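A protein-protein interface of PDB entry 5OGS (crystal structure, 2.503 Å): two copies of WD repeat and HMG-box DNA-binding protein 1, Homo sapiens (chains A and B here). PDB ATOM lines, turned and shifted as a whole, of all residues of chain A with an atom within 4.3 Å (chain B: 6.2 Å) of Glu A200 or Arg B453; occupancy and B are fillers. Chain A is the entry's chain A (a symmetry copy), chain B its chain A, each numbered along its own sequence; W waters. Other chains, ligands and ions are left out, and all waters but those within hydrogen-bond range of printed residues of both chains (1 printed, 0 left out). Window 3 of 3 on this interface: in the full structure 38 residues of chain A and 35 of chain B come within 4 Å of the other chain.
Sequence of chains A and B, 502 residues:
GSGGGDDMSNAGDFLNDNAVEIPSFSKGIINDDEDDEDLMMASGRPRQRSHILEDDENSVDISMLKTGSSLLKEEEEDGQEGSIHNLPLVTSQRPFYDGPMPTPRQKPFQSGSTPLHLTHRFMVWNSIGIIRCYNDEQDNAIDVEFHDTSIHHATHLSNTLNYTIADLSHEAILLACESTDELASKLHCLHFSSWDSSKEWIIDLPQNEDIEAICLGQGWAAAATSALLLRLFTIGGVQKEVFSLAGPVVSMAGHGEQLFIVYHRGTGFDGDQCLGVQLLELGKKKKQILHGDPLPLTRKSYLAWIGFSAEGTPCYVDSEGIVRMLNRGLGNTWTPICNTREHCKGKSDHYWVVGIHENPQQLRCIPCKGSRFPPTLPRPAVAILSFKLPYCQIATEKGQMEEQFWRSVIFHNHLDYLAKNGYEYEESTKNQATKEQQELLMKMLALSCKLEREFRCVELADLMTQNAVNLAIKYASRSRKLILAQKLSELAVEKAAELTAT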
ATOM      1  N   HIS A 188     -12.395   5.550  28.746  1.00  0.00           N
ATOM      2  CA  HIS A 188     -11.482   6.329  27.922  1.00  0.00           C
ATOM      3  C   HIS A 188     -10.813   7.395  28.777  1.00  0.00           C
ATOM      4  O   HIS A 188     -11.493   8.141  29.489  1.00  0.00           O
ATOM      5  CB  HIS A 188     -12.230   6.972  26.749  1.00  0.00           C
ATOM      6  CG  HIS A 188     -11.336   7.641  25.752  1.00  0.00           C
ATOM      7  ND1 HIS A 188     -11.824   8.428  24.731  1.00  0.00           N
ATOM      8  CD2 HIS A 188      -9.990   7.640  25.615  1.00  0.00           C
ATOM      9  CE1 HIS A 188     -10.816   8.885  24.009  1.00  0.00           C
ATOM     10  NE2 HIS A 188      -9.692   8.421  24.525  1.00  0.00           N
ATOM     11  N   CYS A 189      -9.487   7.467  28.701  1.00  0.00           N
ATOM     12  CA  CYS A 189      -8.703   8.419  29.475  1.00  0.00           C
ATOM     13  C   CYS A 189      -7.840   9.252  28.541  1.00  0.00           C
ATOM     14  O   CYS A 189      -7.077   8.704  27.738  1.00  0.00           O
ATOM     15  CB  CYS A 189      -7.827   7.703  30.505  1.00  0.00           C
ATOM     16  SG  CYS A 189      -6.710   8.785  31.424  1.00  0.00           S
ATOM     17  N   ASP A 196       5.061  11.866  27.946  1.00  0.00           N
ATOM     18  CA  ASP A 196       5.436  11.076  26.781  1.00  0.00           C
ATOM     19  C   ASP A 196       4.491  11.385  25.621  1.00  0.00           C
ATOM     20  O   ASP A 196       3.586  12.217  25.725  1.00  0.00           O
ATOM     21  CB  ASP A 196       5.453   9.581  27.116  1.00  0.00           C
ATOM     22  CG  ASP A 196       4.073   9.023  27.429  1.00  0.00           C
ATOM     23  OD1 ASP A 196       3.122   9.810  27.613  1.00  0.00           O
ATOM     24  OD2 ASP A 196       3.943   7.782  27.491  1.00  0.00           O
ATOM     25  N   SER A 198       2.310   9.399  24.222  1.00  0.00           N
ATOM     26  CA  SER A 198       1.072   8.621  24.244  1.00  0.00           C
ATOM     27  C   SER A 198       0.170   9.213  25.322  1.00  0.00           C
ATOM     28  O   SER A 198       0.328   8.916  26.510  1.00  0.00           O
ATOM     29  CB  SER A 198       1.357   7.144  24.499  1.00  0.00           C
ATOM     30  OG  SER A 198       1.899   6.944  25.792  1.00  0.00           O
ATOM     31  N   LYS A 199      -0.779  10.046  24.902  1.00  0.00           N
ATOM     32  CA  LYS A 199      -1.678  10.752  25.809  1.00  0.00           C
ATOM     33  C   LYS A 199      -3.118  10.263  25.674  1.00  0.00           C
ATOM     34  O   LYS A 199      -4.063  11.052  25.724  1.00  0.00           O
ATOM     35  CB  LYS A 199      -1.609  12.258  25.572  1.00  0.00           C
ATOM     36  CG  LYS A 199      -0.250  12.875  25.862  1.00  0.00           C
ATOM     37  CD  LYS A 199      -0.315  14.393  25.794  1.00  0.00           C
ATOM     38  CE  LYS A 199       1.026  15.022  26.132  1.00  0.00           C
ATOM     39  NZ  LYS A 199       0.948  16.509  26.168  1.00  0.00           N
ATOM     40  N   GLU A 200      -3.301   8.954  25.513  1.00  0.00           N
ATOM     41  CA  GLU A 200      -4.635   8.402  25.320  1.00  0.00           C
ATOM     42  C   GLU A 200      -4.589   6.895  25.521  1.00  0.00           C
ATOM     43  O   GLU A 200      -3.633   6.239  25.100  1.00  0.00           O
ATOM     44  CB  GLU A 200      -5.167   8.727  23.918  1.00  0.00           C
ATOM     45  CG  GLU A 200      -6.587   9.260  23.898  1.00  0.00           C
ATOM     46  CD  GLU A 200      -7.110   9.459  22.489  1.00  0.00           C
ATOM     47  OE1 GLU A 200      -6.597   8.795  21.563  1.00  0.00           O
ATOM     48  OE2 GLU A 200      -8.032  10.282  22.306  1.00  0.00           O
ATOM     49  N   TRP A 201      -5.624   6.358  26.165  1.00  0.00           N
ATOM     50  CA  TRP A 201      -5.816   4.915  26.223  1.00  0.00           C
ATOM     51  C   TRP A 201      -7.283   4.625  26.491  1.00  0.00           C
ATOM     52  O   TRP A 201      -7.995   5.438  27.088  1.00  0.00           O
ATOM     53  CB  TRP A 201      -4.927   4.246  27.283  1.00  0.00           C
ATOM     54  CG  TRP A 201      -5.138   4.705  28.702  1.00  0.00           C
ATOM     55  CD1 TRP A 201      -4.386   5.618  29.386  1.00  0.00           C
ATOM     56  CD2 TRP A 201      -6.146   4.253  29.617  1.00  0.00           C
ATOM     57  NE1 TRP A 201      -4.870   5.769  30.663  1.00  0.00           N
ATOM     58  CE2 TRP A 201      -5.949   4.942  30.831  1.00  0.00           C
ATOM     59  CE3 TRP A 201      -7.199   3.337  29.527  1.00  0.00           C
ATOM     60  CZ2 TRP A 201      -6.766   4.746  31.944  1.00  0.00           C
ATOM     61  CZ3 TRP A 201      -8.010   3.145  30.633  1.00  0.00           C
ATOM     62  CH2 TRP A 201      -7.789   3.847  31.825  1.00  0.00           C
ATOM     63  N   LEU B 445       6.581  -4.087  31.429  1.00  0.00           N
ATOM     64  CA  LEU B 445       7.324  -2.863  31.147  1.00  0.00           C
ATOM     65  C   LEU B 445       7.919  -2.896  29.745  1.00  0.00           C
ATOM     66  O   LEU B 445       7.891  -1.888  29.031  1.00  0.00           O
ATOM     67  CB  LEU B 445       8.418  -2.655  32.197  1.00  0.00           C
ATOM     68  CG  LEU B 445       9.302  -1.411  32.062  1.00  0.00           C
ATOM     69  CD1 LEU B 445       9.539  -0.773  33.423  1.00  0.00           C
ATOM     70  CD2 LEU B 445      10.631  -1.752  31.401  1.00  0.00           C
ATOM     71  N   LEU B 447       6.675  -4.493  27.257  1.00  0.00           N
ATOM     72  CA  LEU B 447       5.562  -4.350  26.323  1.00  0.00           C
ATOM     73  C   LEU B 447       5.135  -2.893  26.204  1.00  0.00           C
ATOM     74  O   LEU B 447       4.898  -2.394  25.098  1.00  0.00           O
ATOM     75  CB  LEU B 447       4.390  -5.225  26.766  1.00  0.00           C
ATOM     76  CG  LEU B 447       3.156  -5.187  25.861  1.00  0.00           C
ATOM     77  CD1 LEU B 447       3.520  -5.620  24.451  1.00  0.00           C
ATOM     78  CD2 LEU B 447       2.050  -6.062  26.422  1.00  0.00           C
ATOM     79  N   SER B 448       5.030  -2.193  27.337  1.00  0.00           N
ATOM     80  CA  SER B 448       4.688  -0.775  27.299  1.00  0.00           C
ATOM     81  C   SER B 448       5.773   0.040  26.611  1.00  0.00           C
ATOM     82  O   SER B 448       5.478   1.063  25.983  1.00  0.00           O
ATOM     83  CB  SER B 448       4.449  -0.253  28.717  1.00  0.00           C
ATOM     84  OG  SER B 448       3.493  -1.046  29.397  1.00  0.00           O
ATOM     85  N   CYS B 449       7.031  -0.394  26.719  1.00  0.00           N
ATOM     86  CA  CYS B 449       8.114   0.305  26.036  1.00  0.00           C
ATOM     87  C   CYS B 449       8.007   0.138  24.525  1.00  0.00           C
ATOM     88  O   CYS B 449       8.270   1.082  23.771  1.00  0.00           O
ATOM     89  CB  CYS B 449       9.462  -0.205  26.546  1.00  0.00           C
ATOM     90  SG  CYS B 449      10.889   0.750  25.992  1.00  0.00           S
ATOM     91  N   LYS B 450       7.620  -1.055  24.065  1.00  0.00           N
ATOM     92  CA  LYS B 450       7.419  -1.273  22.636  1.00  0.00           C
ATOM     93  C   LYS B 450       6.269  -0.433  22.098  1.00  0.00           C
ATOM     94  O   LYS B 450       6.306   0.003  20.941  1.00  0.00           O
ATOM     95  CB  LYS B 450       7.164  -2.755  22.362  1.00  0.00           C
ATOM     96  CG  LYS B 450       8.409  -3.624  22.383  1.00  0.00           C
ATOM     97  CD  LYS B 450       8.050  -5.099  22.484  1.00  0.00           C
ATOM     98  CE  LYS B 450       6.961  -5.481  21.490  1.00  0.00           C
ATOM     99  NZ  LYS B 450       7.365  -5.222  20.081  1.00  0.00           N
ATOM    100  N   LEU B 451       5.242  -0.199  22.912  1.00  0.00           N
ATOM    101  CA  LEU B 451       4.089   0.594  22.509  1.00  0.00           C
ATOM    102  C   LEU B 451       4.313   2.091  22.675  1.00  0.00           C
ATOM    103  O   LEU B 451       3.353   2.860  22.552  1.00  0.00           O
ATOM    104  CB  LEU B 451       2.855   0.165  23.306  1.00  0.00           C
ATOM    105  CG  LEU B 451       2.427  -1.295  23.150  1.00  0.00           C
ATOM    106  CD1 LEU B 451       1.234  -1.601  24.041  1.00  0.00           C
ATOM    107  CD2 LEU B 451       2.109  -1.603  21.694  1.00  0.00           C
ATOM    108  N   GLU B 452       5.549   2.513  22.952  1.00  0.00           N
ATOM    109  CA  GLU B 452       5.888   3.918  23.174  1.00  0.00           C
ATOM    110  C   GLU B 452       5.062   4.535  24.300  1.00  0.00           C
ATOM    111  O   GLU B 452       4.733   5.724  24.264  1.00  0.00           O
ATOM    112  CB  GLU B 452       5.740   4.740  21.889  1.00  0.00           C
ATOM    113  CG  GLU B 452       6.727   4.355  20.800  1.00  0.00           C
ATOM    114  CD  GLU B 452       6.540   5.161  19.530  1.00  0.00           C
ATOM    115  OE1 GLU B 452       5.454   5.753  19.353  1.00  0.00           O
ATOM    116  OE2 GLU B 452       7.481   5.203  18.709  1.00  0.00           O
ATOM    117  N   ARG B 453       4.721   3.738  25.310  1.00  0.00           N
ATOM    118  CA  ARG B 453       4.018   4.215  26.498  1.00  0.00           C
ATOM    119  C   ARG B 453       5.023   4.241  27.646  1.00  0.00           C
ATOM    120  O   ARG B 453       5.074   3.339  28.484  1.00  0.00           O
ATOM    121  CB  ARG B 453       2.806   3.338  26.814  1.00  0.00           C
ATOM    122  CG  ARG B 453       1.739   3.364  25.734  1.00  0.00           C
ATOM    123  CD  ARG B 453       0.500   2.604  26.167  1.00  0.00           C
ATOM    124  NE  ARG B 453      -0.581   2.717  25.194  1.00  0.00           N
ATOM    125  CZ  ARG B 453      -1.461   3.713  25.167  1.00  0.00           C
ATOM    126  NH1 ARG B 453      -1.385   4.692  26.059  1.00  0.00           N
ATOM    127  NH2 ARG B 453      -2.414   3.733  24.246  1.00  0.00           N
ATOM    128  N   GLU B 454       5.834   5.299  27.676  1.00  0.00           N
ATOM    129  CA  GLU B 454       6.916   5.389  28.647  1.00  0.00           C
ATOM    130  C   GLU B 454       6.422   5.814  30.024  1.00  0.00           C
ATOM    131  O   GLU B 454       7.029   5.441  31.034  1.00  0.00           O
ATOM    132  CB  GLU B 454       7.986   6.354  28.139  1.00  0.00           C
ATOM    133  CG  GLU B 454       8.439   6.046  26.720  1.00  0.00           C
ATOM    134  CD  GLU B 454       9.461   7.033  26.198  1.00  0.00           C
ATOM    135  OE1 GLU B 454       9.908   7.902  26.977  1.00  0.00           O
ATOM    136  OE2 GLU B 454       9.818   6.939  25.005  1.00  0.00           O
ATOM    137  N   PHE B 455       5.337   6.590  30.087  1.00  0.00           N
ATOM    138  CA  PHE B 455       4.741   6.909  31.380  1.00  0.00           C
ATOM    139  C   PHE B 455       4.210   5.650  32.054  1.00  0.00           C
ATOM    140  O   PHE B 455       4.344   5.482  33.272  1.00  0.00           O
ATOM    141  CB  PHE B 455       3.624   7.940  31.206  1.00  0.00           C
ATOM    142  CG  PHE B 455       3.068   8.463  32.504  1.00  0.00           C
ATOM    143  CD1 PHE B 455       3.527   9.657  33.037  1.00  0.00           C
ATOM    144  CD2 PHE B 455       2.086   7.765  33.188  1.00  0.00           C
ATOM    145  CE1 PHE B 455       3.020  10.141  34.229  1.00  0.00           C
ATOM    146  CE2 PHE B 455       1.580   8.242  34.380  1.00  0.00           C
ATOM    147  CZ  PHE B 455       2.044   9.433  34.901  1.00  0.00           C
ATOM    148  N   ARG B 456       3.606   4.753  31.272  1.00  0.00           N
ATOM    149  CA  ARG B 456       3.119   3.492  31.817  1.00  0.00           C
ATOM    150  C   ARG B 456       4.263   2.633  32.342  1.00  0.00           C
ATOM    151  O   ARG B 456       4.082   1.886  33.310  1.00  0.00           O
ATOM    152  CB  ARG B 456       2.326   2.742  30.745  1.00  0.00           C
ATOM    153  CG  ARG B 456       1.759   1.409  31.192  1.00  0.00           C
ATOM    154  CD  ARG B 456       0.929   0.762  30.094  1.00  0.00           C
ATOM    155  NE  ARG B 456      -0.280   1.523  29.788  1.00  0.00           N
ATOM    156  CZ  ARG B 456      -1.128   1.213  28.813  1.00  0.00           C
ATOM    157  NH1 ARG B 456      -0.898   0.160  28.042  1.00  0.00           N
ATOM    158  NH2 ARG B 456      -2.204   1.960  28.604  1.00  0.00           N
ATOM    159  N   CYS B 457       5.443   2.730  31.726  1.00  0.00           N
ATOM    160  CA  CYS B 457       6.592   1.970  32.207  1.00  0.00           C
ATOM    161  C   CYS B 457       6.985   2.397  33.615  1.00  0.00           C
ATOM    162  O   CYS B 457       7.313   1.554  34.460  1.00  0.00           O
ATOM    163  CB  CYS B 457       7.774   2.135  31.250  1.00  0.00           C
ATOM    164  SG  CYS B 457       7.504   1.469  29.595  1.00  0.00           S
ATOM    165  N   VAL B 458       6.957   3.704  33.888  1.00  0.00           N
ATOM    166  CA  VAL B 458       7.304   4.194  35.218  1.00  0.00           C
ATOM    167  C   VAL B 458       6.270   3.739  36.240  1.00  0.00           C
ATOM    168  O   VAL B 458       6.611   3.423  37.387  1.00  0.00           O
ATOM    169  CB  VAL B 458       7.451   5.727  35.200  1.00  0.00           C
ATOM    170  CG1 VAL B 458       7.802   6.250  36.587  1.00  0.00           C
ATOM    171  CG2 VAL B 458       8.504   6.146  34.188  1.00  0.00           C
ATOM    172  N   LYS B 481      15.929   5.248  25.086  1.00  0.00           N
ATOM    173  CA  LYS B 481      14.820   5.867  25.811  1.00  0.00           C
ATOM    174  C   LYS B 481      15.389   6.714  26.950  1.00  0.00           C
ATOM    175  O   LYS B 481      15.335   6.363  28.129  1.00  0.00           O
ATOM    176  CB  LYS B 481      13.849   4.806  26.323  1.00  0.00           C
ATOM    177  CG  LYS B 481      13.242   3.929  25.235  1.00  0.00           C
ATOM    178  CD  LYS B 481      12.149   4.657  24.480  1.00  0.00           C
ATOM    179  CE  LYS B 481      11.417   3.706  23.549  1.00  0.00           C
ATOM    180  NZ  LYS B 481      10.276   4.365  22.861  1.00  0.00           N
HETATM  181  O   HOH W   1       2.564   5.961  28.851  1.00  0.00           O
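The side-chain carboxylate (OD2) of Asp A196 is in hydrogen-bond range of the backbone NH (N) of Phe B455, at 3.2 Å.
NH1 of Arg B453 lies within hydrogen-bond range of O of Glu A200 (2.9 Å).
The side-chain hydroxyl (OG) of Ser A198 lies within hydrogen-bond range of the backbone carbonyl oxygen (O) of Glu B452 (3.4 Å).
N of Glu B454 is in hydrogen-bond range of OD2 of Asp A196, 3.1 Å away.
The backbone NH (N) of Cys A189 sits at hydrogen-bond distance from the backbone carbonyl oxygen (O) of Trp A201 (3.0 Å).
The side-chain hydroxyl (OG) of Ser A198 is in hydrogen-bond range of the side-chain carboxylate (OD2) of Asp A196.
The backbone NH (N) of Arg B453 sits at hydrogen-bond distance from the backbone carbonyl oxygen (O) of Ser B448, at 2.9 Å.
O of Arg B453 lies within hydrogen-bond range of SG of Cys B457, at 3.3 Å.
OE2 of Glu B454 is in salt-bridge range of NZ of Lys B481 (3.4 Å).
NE2 of His A188 lies close to OE2 of Glu A200, 3.3 Å away.
Among the printed residues, pairs that only touch across the chains: Ser A198 with Arg B453, Asp A196 with Arg B453, Trp A201 with Arg B453, Trp A201 with Arg B456 and Asp A196 with Glu B452.
Of the printed residues of chain A, Glu B452 touches Asp A196 and Ser A198.
Printed residues of chain A within 4 Å of Arg B456: Trp A201 (3.8 Å).
Printed residues of chain B within 4 Å of Trp A201: Arg B453 and Arg B456.
Of the printed residues of chain A, Glu B454 touches Asp A196.
Cys B449 touches none of the printed residues of chain A.
Cys A189 touches none of the printed residues of chain B.
The nearest residue of chain B that does not touch Glu A200 is Arg B456 (5.7 Å).
The nearest printed residue of chain A that does not touch Arg B456 is Asp A196 (4.9 Å).
Hydrophobic or aromatic side chains of chain A that line the printed part of chain B: Trp A201.
Hydrophobic or aromatic side chains of chain B that line the printed part of chain A: Phe B455.
Among the printed residues, 9 pairs touch across the chains.
No position is printed for both chains.
Water W1 lies within hydrogen-bond range of OD2 of Asp A196 (2.7 Å), N of Arg B456 (2.9 Å), N of Phe B455 (3.1 Å) and OG of Ser A198 (3.3 Å).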
